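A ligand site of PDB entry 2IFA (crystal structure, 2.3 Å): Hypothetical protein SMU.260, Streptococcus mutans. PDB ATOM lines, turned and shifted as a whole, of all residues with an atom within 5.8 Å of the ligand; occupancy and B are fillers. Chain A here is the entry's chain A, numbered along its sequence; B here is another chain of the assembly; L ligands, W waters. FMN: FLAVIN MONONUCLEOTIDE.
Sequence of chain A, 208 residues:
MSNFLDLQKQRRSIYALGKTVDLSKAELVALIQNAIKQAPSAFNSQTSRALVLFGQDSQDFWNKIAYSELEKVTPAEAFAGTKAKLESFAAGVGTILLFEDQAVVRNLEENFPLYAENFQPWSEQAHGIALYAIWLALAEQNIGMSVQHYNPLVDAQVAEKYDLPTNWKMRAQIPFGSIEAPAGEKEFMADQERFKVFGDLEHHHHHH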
ATOM      1  N   ARG A  11     -27.386 -19.406  10.129  1.00  0.00           N
ATOM      2  CA  ARG A  11     -27.477 -18.764  11.447  1.00  0.00           C
ATOM      3  C   ARG A  11     -27.359 -17.256  11.374  1.00  0.00           C
ATOM      4  O   ARG A  11     -26.353 -16.725  10.884  1.00  0.00           O
ATOM      5  CB  ARG A  11     -26.355 -19.262  12.376  1.00  0.00           C
ATOM      6  CG  ARG A  11     -26.435 -18.687  13.790  1.00  0.00           C
ATOM      7  CD  ARG A  11     -25.056 -18.442  14.387  1.00  0.00           C
ATOM      8  NE  ARG A  11     -24.307 -17.441  13.623  1.00  0.00           N
ATOM      9  CZ  ARG A  11     -24.651 -16.163  13.509  1.00  0.00           C
ATOM     10  NH1 ARG A  11     -25.737 -15.705  14.114  1.00  0.00           N
ATOM     11  NH2 ARG A  11     -23.908 -15.342  12.767  1.00  0.00           N
ATOM     12  N   ARG A  12     -28.389 -16.571  11.866  1.00  0.00           N
ATOM     13  CA  ARG A  12     -28.417 -15.116  11.859  1.00  0.00           C
ATOM     14  C   ARG A  12     -29.094 -14.644  13.149  1.00  0.00           C
ATOM     15  O   ARG A  12     -29.632 -15.444  13.895  1.00  0.00           O
ATOM     16  CB  ARG A  12     -29.224 -14.614  10.648  1.00  0.00           C
ATOM     17  CG  ARG A  12     -28.579 -14.873   9.272  1.00  0.00           C
ATOM     18  CD  ARG A  12     -27.192 -14.231   9.164  1.00  0.00           C
ATOM     19  NE  ARG A  12     -27.277 -12.795   9.383  1.00  0.00           N
ATOM     20  CZ  ARG A  12     -27.855 -11.938   8.544  1.00  0.00           C
ATOM     21  NH1 ARG A  12     -28.410 -12.367   7.414  1.00  0.00           N
ATOM     22  NH2 ARG A  12     -27.917 -10.658   8.862  1.00  0.00           N
ATOM     23  N   SER A  13     -29.040 -13.337  13.418  1.00  0.00           N
ATOM     24  CA  SER A  13     -29.707 -12.813  14.603  1.00  0.00           C
ATOM     25  C   SER A  13     -31.167 -12.558  14.212  1.00  0.00           C
ATOM     26  O   SER A  13     -31.423 -11.816  13.273  1.00  0.00           O
ATOM     27  CB  SER A  13     -29.065 -11.506  15.058  1.00  0.00           C
ATOM     28  OG  SER A  13     -27.895 -11.744  15.820  1.00  0.00           O
ATOM     29  N   TYR A  15     -34.820 -11.169  15.471  1.00  0.00           N
ATOM     30  CA  TYR A  15     -35.529 -10.336  16.424  1.00  0.00           C
ATOM     31  C   TYR A  15     -37.055 -10.508  16.375  1.00  0.00           C
ATOM     32  O   TYR A  15     -37.767  -9.966  17.211  1.00  0.00           O
ATOM     33  CB  TYR A  15     -35.133  -8.867  16.233  1.00  0.00           C
ATOM     34  CG  TYR A  15     -33.658  -8.613  16.469  1.00  0.00           C
ATOM     35  CD1 TYR A  15     -33.132  -8.681  17.767  1.00  0.00           C
ATOM     36  CD2 TYR A  15     -32.784  -8.368  15.412  1.00  0.00           C
ATOM     37  CE1 TYR A  15     -31.774  -8.512  17.989  1.00  0.00           C
ATOM     38  CE2 TYR A  15     -31.415  -8.207  15.629  1.00  0.00           C
ATOM     39  CZ  TYR A  15     -30.920  -8.274  16.918  1.00  0.00           C
ATOM     40  OH  TYR A  15     -29.567  -8.153  17.164  1.00  0.00           O
ATOM     41  N   LEU A 131     -22.073 -19.890  23.530  1.00  0.00           N
ATOM     42  CA  LEU A 131     -23.109 -19.109  22.852  1.00  0.00           C
ATOM     43  C   LEU A 131     -23.251 -19.521  21.392  1.00  0.00           C
ATOM     44  O   LEU A 131     -24.356 -19.731  20.906  1.00  0.00           O
ATOM     45  CB  LEU A 131     -22.768 -17.615  22.911  1.00  0.00           C
ATOM     46  CG  LEU A 131     -23.627 -16.639  22.113  1.00  0.00           C
ATOM     47  CD1 LEU A 131     -24.959 -16.391  22.825  1.00  0.00           C
ATOM     48  CD2 LEU A 131     -22.881 -15.323  21.954  1.00  0.00           C
ATOM     49  N   TRP A 135     -26.379 -21.276  19.406  1.00  0.00           N
ATOM     50  CA  TRP A 135     -26.885 -20.548  18.249  1.00  0.00           C
ATOM     51  C   TRP A 135     -26.897 -21.465  17.008  1.00  0.00           C
ATOM     52  O   TRP A 135     -27.829 -21.464  16.207  1.00  0.00           O
ATOM     53  CB  TRP A 135     -25.986 -19.342  17.982  1.00  0.00           C
ATOM     54  CG  TRP A 135     -26.712 -18.120  17.504  1.00  0.00           C
ATOM     55  CD1 TRP A 135     -27.914 -18.076  16.880  1.00  0.00           C
ATOM     56  CD2 TRP A 135     -26.271 -16.753  17.624  1.00  0.00           C
ATOM     57  NE1 TRP A 135     -28.267 -16.781  16.603  1.00  0.00           N
ATOM     58  CE2 TRP A 135     -27.274 -15.943  17.045  1.00  0.00           C
ATOM     59  CE3 TRP A 135     -25.129 -16.138  18.167  1.00  0.00           C
ATOM     60  CZ2 TRP A 135     -27.173 -14.550  16.992  1.00  0.00           C
ATOM     61  CZ3 TRP A 135     -25.039 -14.738  18.119  1.00  0.00           C
ATOM     62  CH2 TRP A 135     -26.054 -13.970  17.535  1.00  0.00           C
ATOM     63  N   SER A 146     -31.622 -14.330  19.543  1.00  0.00           N
ATOM     64  CA  SER A 146     -30.756 -13.161  19.554  1.00  0.00           C
ATOM     65  C   SER A 146     -30.007 -13.203  20.893  1.00  0.00           C
ATOM     66  O   SER A 146     -30.390 -13.947  21.796  1.00  0.00           O
ATOM     67  CB  SER A 146     -31.570 -11.876  19.449  1.00  0.00           C
ATOM     68  OG  SER A 146     -32.120 -11.523  20.699  1.00  0.00           O
ATOM     69  N   VAL A 147     -28.935 -12.436  21.022  1.00  0.00           N
ATOM     70  CA  VAL A 147     -28.182 -12.431  22.269  1.00  0.00           C
ATOM     71  C   VAL A 147     -28.395 -11.072  22.909  1.00  0.00           C
ATOM     72  O   VAL A 147     -28.265 -10.040  22.260  1.00  0.00           O
ATOM     73  CB  VAL A 147     -26.668 -12.675  22.006  1.00  0.00           C
ATOM     74  CG1 VAL A 147     -25.928 -12.920  23.332  1.00  0.00           C
ATOM     75  CG2 VAL A 147     -26.510 -13.858  21.106  1.00  0.00           C
ATOM     76  N   GLN A 148     -28.755 -11.063  24.185  1.00  0.00           N
ATOM     77  CA  GLN A 148     -29.008  -9.806  24.878  1.00  0.00           C
ATOM     78  C   GLN A 148     -28.078  -9.598  26.060  1.00  0.00           C
ATOM     79  O   GLN A 148     -27.550 -10.558  26.634  1.00  0.00           O
ATOM     80  CB  GLN A 148     -30.466  -9.745  25.346  1.00  0.00           C
ATOM     81  CG  GLN A 148     -31.502  -9.720  24.222  1.00  0.00           C
ATOM     82  CD  GLN A 148     -31.256  -8.609  23.205  1.00  0.00           C
ATOM     83  OE1 GLN A 148     -31.084  -7.443  23.558  1.00  0.00           O
ATOM     84  NE2 GLN A 148     -31.250  -8.976  21.929  1.00  0.00           N
ATOM     85  N   HIS A 149     -27.870  -8.336  26.433  1.00  0.00           N
ATOM     86  CA  HIS A 149     -27.014  -8.027  27.552  1.00  0.00           C
ATOM     87  C   HIS A 149     -27.591  -7.017  28.534  1.00  0.00           C
ATOM     88  O   HIS A 149     -27.116  -5.888  28.671  1.00  0.00           O
ATOM     89  CB  HIS A 149     -25.629  -7.596  27.051  1.00  0.00           C
ATOM     90  CG  HIS A 149     -24.858  -8.707  26.412  1.00  0.00           C
ATOM     91  ND1 HIS A 149     -24.862  -8.933  25.048  1.00  0.00           N
ATOM     92  CD2 HIS A 149     -24.136  -9.724  26.957  1.00  0.00           C
ATOM     93  CE1 HIS A 149     -24.184 -10.027  24.781  1.00  0.00           C
ATOM     94  NE2 HIS A 149     -23.738 -10.527  25.919  1.00  0.00           N
ATOM     95  N   ALA A 183     -33.670 -12.225   8.658  1.00  0.00           N
ATOM     96  CA  ALA A 183     -32.788 -11.092   8.925  1.00  0.00           C
ATOM     97  C   ALA A 183     -32.471 -10.383   7.625  1.00  0.00           C
ATOM     98  O   ALA A 183     -32.702 -10.922   6.543  1.00  0.00           O
ATOM     99  CB  ALA A 183     -31.499 -11.583   9.563  1.00  0.00           C
ATOM    100  N   LYS A 186     -26.430  -8.690   5.694  1.00  0.00           N
ATOM    101  CA  LYS A 186     -25.318  -8.439   6.604  1.00  0.00           C
ATOM    102  C   LYS A 186     -24.106  -7.989   5.798  1.00  0.00           C
ATOM    103  O   LYS A 186     -23.902  -8.420   4.672  1.00  0.00           O
ATOM    104  CB  LYS A 186     -24.992  -9.720   7.378  1.00  0.00           C
ATOM    105  CG  LYS A 186     -23.899  -9.544   8.416  1.00  0.00           C
ATOM    106  CD  LYS A 186     -23.771 -10.790   9.287  1.00  0.00           C
ATOM    107  CE  LYS A 186     -23.475 -12.030   8.470  1.00  0.00           C
ATOM    108  NZ  LYS A 186     -23.348 -13.221   9.360  1.00  0.00           N
ATOM    109  N   GLN B  38     -18.184 -15.836   8.883  1.00  0.00           N
ATOM    110  CA  GLN B  38     -19.527 -16.162   9.307  1.00  0.00           C
ATOM    111  C   GLN B  38     -19.673 -16.168  10.828  1.00  0.00           C
ATOM    112  O   GLN B  38     -20.787 -16.133  11.342  1.00  0.00           O
ATOM    113  CB  GLN B  38     -19.922 -17.526   8.733  1.00  0.00           C
ATOM    114  CG  GLN B  38     -20.869 -17.421   7.535  1.00  0.00           C
ATOM    115  CD  GLN B  38     -20.312 -16.604   6.402  1.00  0.00           C
ATOM    116  OE1 GLN B  38     -21.051 -16.089   5.565  1.00  0.00           O
ATOM    117  NE2 GLN B  38     -18.984 -16.475   6.367  1.00  0.00           N
ATOM    118  N   PRO B  40     -20.088 -14.678  14.219  1.00  0.00           N
ATOM    119  CA  PRO B  40     -20.589 -13.386  14.704  1.00  0.00           C
ATOM    120  C   PRO B  40     -19.736 -12.649  15.716  1.00  0.00           C
ATOM    121  O   PRO B  40     -18.905 -13.225  16.391  1.00  0.00           O
ATOM    122  CB  PRO B  40     -21.972 -13.759  15.269  1.00  0.00           C
ATOM    123  CG  PRO B  40     -21.722 -15.127  15.821  1.00  0.00           C
ATOM    124  CD  PRO B  40     -20.916 -15.789  14.726  1.00  0.00           C
ATOM    125  N   SER B  41     -19.998 -11.358  15.830  1.00  0.00           N
ATOM    126  CA  SER B  41     -19.279 -10.500  16.775  1.00  0.00           C
ATOM    127  C   SER B  41     -20.203  -9.356  17.176  1.00  0.00           C
ATOM    128  O   SER B  41     -21.117  -8.977  16.428  1.00  0.00           O
ATOM    129  CB  SER B  41     -18.043  -9.898  16.129  1.00  0.00           C
ATOM    130  OG  SER B  41     -18.447  -8.997  15.110  1.00  0.00           O
ATOM    131  N   ALA B  42     -19.957  -8.822  18.370  1.00  0.00           N
ATOM    132  CA  ALA B  42     -20.728  -7.709  18.914  1.00  0.00           C
ATOM    133  C   ALA B  42     -20.981  -6.642  17.854  1.00  0.00           C
ATOM    134  O   ALA B  42     -20.037  -6.010  17.351  1.00  0.00           O
ATOM    135  CB  ALA B  42     -19.976  -7.096  20.090  1.00  0.00           C
ATOM    136  N   PHE B  43     -22.261  -6.440  17.555  1.00  0.00           N
ATOM    137  CA  PHE B  43     -22.748  -5.504  16.540  1.00  0.00           C
ATOM    138  C   PHE B  43     -21.887  -5.474  15.299  1.00  0.00           C
ATOM    139  O   PHE B  43     -21.533  -4.419  14.786  1.00  0.00           O
ATOM    140  CB  PHE B  43     -22.941  -4.107  17.120  1.00  0.00           C
ATOM    141  CG  PHE B  43     -21.775  -3.595  17.876  1.00  0.00           C
ATOM    142  CD1 PHE B  43     -20.687  -3.022  17.225  1.00  0.00           C
ATOM    143  CD2 PHE B  43     -21.738  -3.739  19.255  1.00  0.00           C
ATOM    144  CE1 PHE B  43     -19.573  -2.602  17.943  1.00  0.00           C
ATOM    145  CE2 PHE B  43     -20.631  -3.323  19.985  1.00  0.00           C
ATOM    146  CZ  PHE B  43     -19.545  -2.763  19.329  1.00  0.00           C
ATOM    147  N   ASN B  44     -21.568  -6.680  14.844  1.00  0.00           N
ATOM    148  CA  ASN B  44     -20.758  -6.876  13.659  1.00  0.00           C
ATOM    149  C   ASN B  44     -19.488  -6.012  13.693  1.00  0.00           C
ATOM    150  O   ASN B  44     -19.108  -5.430  12.699  1.00  0.00           O
ATOM    151  CB  ASN B  44     -21.618  -6.561  12.414  1.00  0.00           C
ATOM    152  CG  ASN B  44     -21.109  -7.270  11.173  1.00  0.00           C
ATOM    153  OD1 ASN B  44     -20.585  -8.376  11.239  1.00  0.00           O
ATOM    154  ND2 ASN B  44     -21.280  -6.630  10.009  1.00  0.00           N
ATOM    155  N   PRO B 121     -14.723  -7.969  27.113  1.00  0.00           N
ATOM    156  CA  PRO B 121     -15.245  -9.332  27.212  1.00  0.00           C
ATOM    157  C   PRO B 121     -15.890  -9.781  25.891  1.00  0.00           C
ATOM    158  O   PRO B 121     -15.765 -10.934  25.490  1.00  0.00           O
ATOM    159  CB  PRO B 121     -16.244  -9.232  28.379  1.00  0.00           C
ATOM    160  CG  PRO B 121     -15.628  -8.179  29.250  1.00  0.00           C
ATOM    161  CD  PRO B 121     -15.176  -7.148  28.253  1.00  0.00           C
ATOM    162  N   TRP B 122     -16.590  -8.880  25.191  1.00  0.00           N
ATOM    163  CA  TRP B 122     -17.218  -9.206  23.904  1.00  0.00           C
ATOM    164  C   TRP B 122     -16.191  -9.548  22.836  1.00  0.00           C
ATOM    165  O   TRP B 122     -16.467 -10.357  21.929  1.00  0.00           O
ATOM    166  CB  TRP B 122     -18.098  -8.032  23.394  1.00  0.00           C
ATOM    167  CG  TRP B 122     -19.397  -7.863  24.098  1.00  0.00           C
ATOM    168  CD1 TRP B 122     -20.012  -8.759  24.929  1.00  0.00           C
ATOM    169  CD2 TRP B 122     -20.251  -6.719  24.042  1.00  0.00           C
ATOM    170  NE1 TRP B 122     -21.199  -8.248  25.395  1.00  0.00           N
ATOM    171  CE2 TRP B 122     -21.374  -6.996  24.867  1.00  0.00           C
ATOM    172  CE3 TRP B 122     -20.189  -5.494  23.366  1.00  0.00           C
ATOM    173  CZ2 TRP B 122     -22.417  -6.081  25.050  1.00  0.00           C
ATOM    174  CZ3 TRP B 122     -21.229  -4.583  23.540  1.00  0.00           C
ATOM    175  CH2 TRP B 122     -22.328  -4.883  24.371  1.00  0.00           C
ATOM    176  N   SER B 123     -15.014  -8.922  22.931  1.00  0.00           N
ATOM    177  CA  SER B 123     -13.925  -9.201  22.000  1.00  0.00           C
ATOM    178  C   SER B 123     -13.379 -10.598  22.282  1.00  0.00           C
ATOM    179  O   SER B 123     -13.226 -11.406  21.361  1.00  0.00           O
ATOM    180  CB  SER B 123     -12.806  -8.178  22.150  1.00  0.00           C
ATOM    181  OG  SER B 123     -11.676  -8.601  21.412  1.00  0.00           O
ATOM    182  N   GLN B 125     -14.928 -12.989  23.718  1.00  0.00           N
ATOM    183  CA  GLN B 125     -15.983 -13.925  23.309  1.00  0.00           C
ATOM    184  C   GLN B 125     -15.993 -14.101  21.777  1.00  0.00           C
ATOM    185  O   GLN B 125     -16.150 -15.218  21.286  1.00  0.00           O
ATOM    186  CB  GLN B 125     -17.362 -13.440  23.813  1.00  0.00           C
ATOM    187  CG  GLN B 125     -17.438 -13.337  25.345  1.00  0.00           C
ATOM    188  CD  GLN B 125     -18.662 -12.566  25.817  1.00  0.00           C
ATOM    189  OE1 GLN B 125     -18.874 -12.360  27.033  1.00  0.00           O
ATOM    190  NE2 GLN B 125     -19.460 -12.128  24.874  1.00  0.00           N
ATOM    191  N   ALA B 126     -15.776 -13.002  21.049  1.00  0.00           N
ATOM    192  CA  ALA B 126     -15.750 -13.068  19.576  1.00  0.00           C
ATOM    193  C   ALA B 126     -14.574 -13.936  19.129  1.00  0.00           C
ATOM    194  O   ALA B 126     -14.703 -14.699  18.171  1.00  0.00           O
ATOM    195  CB  ALA B 126     -15.632 -11.677  18.981  1.00  0.00           C
ATOM    196  N   ILE B 129     -15.424 -17.552  19.533  1.00  0.00           N
ATOM    197  CA  ILE B 129     -16.359 -17.905  18.471  1.00  0.00           C
ATOM    198  C   ILE B 129     -15.657 -18.201  17.144  1.00  0.00           C
ATOM    199  O   ILE B 129     -16.047 -19.103  16.402  1.00  0.00           O
ATOM    200  CB  ILE B 129     -17.379 -16.771  18.267  1.00  0.00           C
ATOM    201  CG1 ILE B 129     -18.256 -16.654  19.531  1.00  0.00           C
ATOM    202  CG2 ILE B 129     -18.200 -17.002  16.990  1.00  0.00           C
ATOM    203  CD1 ILE B 129     -19.327 -15.591  19.453  1.00  0.00           C
HETATM  204  N1  FMN L   1     -27.103  -8.381  19.435  1.00  0.00           N
HETATM  205  C2  FMN L   1     -28.019  -7.564  20.102  1.00  0.00           C
HETATM  206  O2  FMN L   1     -29.103  -7.261  19.646  1.00  0.00           O
HETATM  207  N3  FMN L   1     -27.591  -7.102  21.399  1.00  0.00           N
HETATM  208  C4  FMN L   1     -26.350  -7.402  22.063  1.00  0.00           C
HETATM  209  O4  FMN L   1     -26.120  -6.941  23.162  1.00  0.00           O
HETATM  210  C4A FMN L   1     -25.475  -8.246  21.363  1.00  0.00           C
HETATM  211  N5  FMN L   1     -24.248  -8.696  21.822  1.00  0.00           N
HETATM  212  C5A FMN L   1     -23.294  -9.540  21.273  1.00  0.00           C
HETATM  213  C6  FMN L   1     -22.047  -9.888  22.010  1.00  0.00           C
HETATM  214  C7  FMN L   1     -21.093 -10.832  21.385  1.00  0.00           C
HETATM  215  C7M FMN L   1     -19.838 -11.175  22.181  1.00  0.00           C
HETATM  216  C8  FMN L   1     -21.408 -11.404  20.016  1.00  0.00           C
HETATM  217  C8M FMN L   1     -20.529 -12.426  19.223  1.00  0.00           C
HETATM  218  C9  FMN L   1     -22.647 -10.996  19.355  1.00  0.00           C
HETATM  219  C9A FMN L   1     -23.618 -10.064  19.957  1.00  0.00           C
HETATM  220  N10 FMN L   1     -24.908  -9.605  19.394  1.00  0.00           N
HETATM  221  C10 FMN L   1     -25.887  -8.735  20.015  1.00  0.00           C
HETATM  222  C1' FMN L   1     -25.259 -10.138  17.982  1.00  0.00           C
HETATM  223  C2' FMN L   1     -24.480  -9.410  16.833  1.00  0.00           C
HETATM  224  O2' FMN L   1     -24.779  -8.021  16.733  1.00  0.00           O
HETATM  225  C3' FMN L   1     -24.811 -10.068  15.503  1.00  0.00           C
HETATM  226  O3' FMN L   1     -24.449 -11.436  15.657  1.00  0.00           O
HETATM  227  C4' FMN L   1     -23.961  -9.506  14.298  1.00  0.00           C
HETATM  228  O4' FMN L   1     -24.406  -8.227  13.839  1.00  0.00           O
HETATM  229  C5' FMN L   1     -24.024 -10.376  13.076  1.00  0.00           C
HETATM  230  O5' FMN L   1     -25.301 -10.617  12.706  1.00  0.00           O
HETATM  231  P   FMN L   1     -25.868 -12.067  12.662  1.00  0.00           P
HETATM  232  O1P FMN L   1     -24.978 -12.844  11.838  1.00  0.00           O
HETATM  233  O2P FMN L   1     -25.929 -12.522  14.058  1.00  0.00           O
HETATM  234  O3P FMN L   1     -27.143 -11.823  12.122  1.00  0.00           O
HETATM  235  O   HOH W   1     -27.398  -7.184  16.056  1.00  0.00           O
HETATM  236  O   HOH W   2     -25.811  -4.520  24.490  1.00  0.00           O
HETATM  237  O   HOH W   3     -25.088  -7.373  11.142  1.00  0.00           O
HETATM  238  O   HOH W   4     -27.650  -8.695  11.639  1.00  0.00           O
HETATM  239  O   HOH W   5     -28.543 -10.874  18.695  1.00  0.00           O
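N of Ser 13 sits at hydrogen-bond distance from O3P of the ligand (2.8 Å).
O3P of the ligand lies within salt-bridge range of NE of Arg 12, 2.9 Å away.
OG of Ser 13 lies within hydrogen-bond range of O2P of the ligand.
N3 of the ligand is in hydrogen-bond range of O of Val 147.
The backbone NH (N) of Phe 43 of chain B is in hydrogen-bond range of an oxygen (O2') of the ligand (3.1 Å).
NH2 of Arg 11 lies within salt-bridge range of O1P of the ligand.
The side-chain hydroxyl of Tyr 15 is in hydrogen-bond range of an oxygen (O2) of the ligand, at 2.7 Å.
O4' of the ligand sits at hydrogen-bond distance from N of Asn 44 of chain B (3.4 Å).
NZ of Lys 186 lies within salt-bridge range of O1P of the ligand (3.0 Å).
ND1 of His 149 sits at hydrogen-bond distance from O4 of the ligand, at 3.0 Å.
A ring nitrogen (NE2) of His 149 sits at hydrogen-bond distance from the indole nitrogen (NE1) of Trp 122 of chain B, at 3.5 Å.
The indole nitrogen of Trp 135 lies within hydrogen-bond range of the backbone carbonyl oxygen of Arg 12 (3.3 Å).
The side-chain amide nitrogen (NE2) of Gln 148 sits at hydrogen-bond distance from the side-chain hydroxyl (OG) of Ser 146 (3.0 Å).
Residues that only touch the ligand: Gln 125 of chain B (2.9 Å), Ser 41 of chain B (3.4 Å), Pro 40 of chain B (3.4 Å), Ala 42 of chain B (3.4 Å), Ile 129 of chain B (3.4 Å), Trp 122 of chain B (3.5 Å), Trp 135 (3.5 Å) and Gln 148 (3.6 Å).
Hydrophobic or aromatic side chains that line the ligand: Tyr 15, Trp 135, His 149, Pro 40 of chain B, Ala 42 of chain B, Trp 122 of chain B and Ile 129 of chain B.
17 residues have an atom within 4 Å of the ligand: Arg 11, Arg 12, Ser 13, Tyr 15, Trp 135, Val 147, Gln 148, His 149, Lys 186, Pro 40 of chain B, Ser 41 of chain B, Ala 42 of chain B, Phe 43 of chain B, Asn 44 of chain B, Trp 122 of chain B, Gln 125 of chain B and Ile 129 of chain B.
The nearest printed residue that does not touch the ligand is Ala 126 of chain B (4.6 Å).
Water W1 lies within hydrogen-bond range of the side-chain hydroxyl of Tyr 15 (2.6 Å) and an oxygen (O2') of the ligand (2.8 Å).
Water W5 lies within hydrogen-bond range of the backbone NH of Val 147 (2.8 Å), a nitrogen (N1) of the ligand (3.0 Å), the side-chain hydroxyl of Ser 13 (3.1 Å) and the side-chain hydroxyl of Tyr 15 (3.3 Å).
Water W4 lies within hydrogen-bond range of O3P of the ligand (3.2 Å) and NH2 of Arg 12 (3.4 Å).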
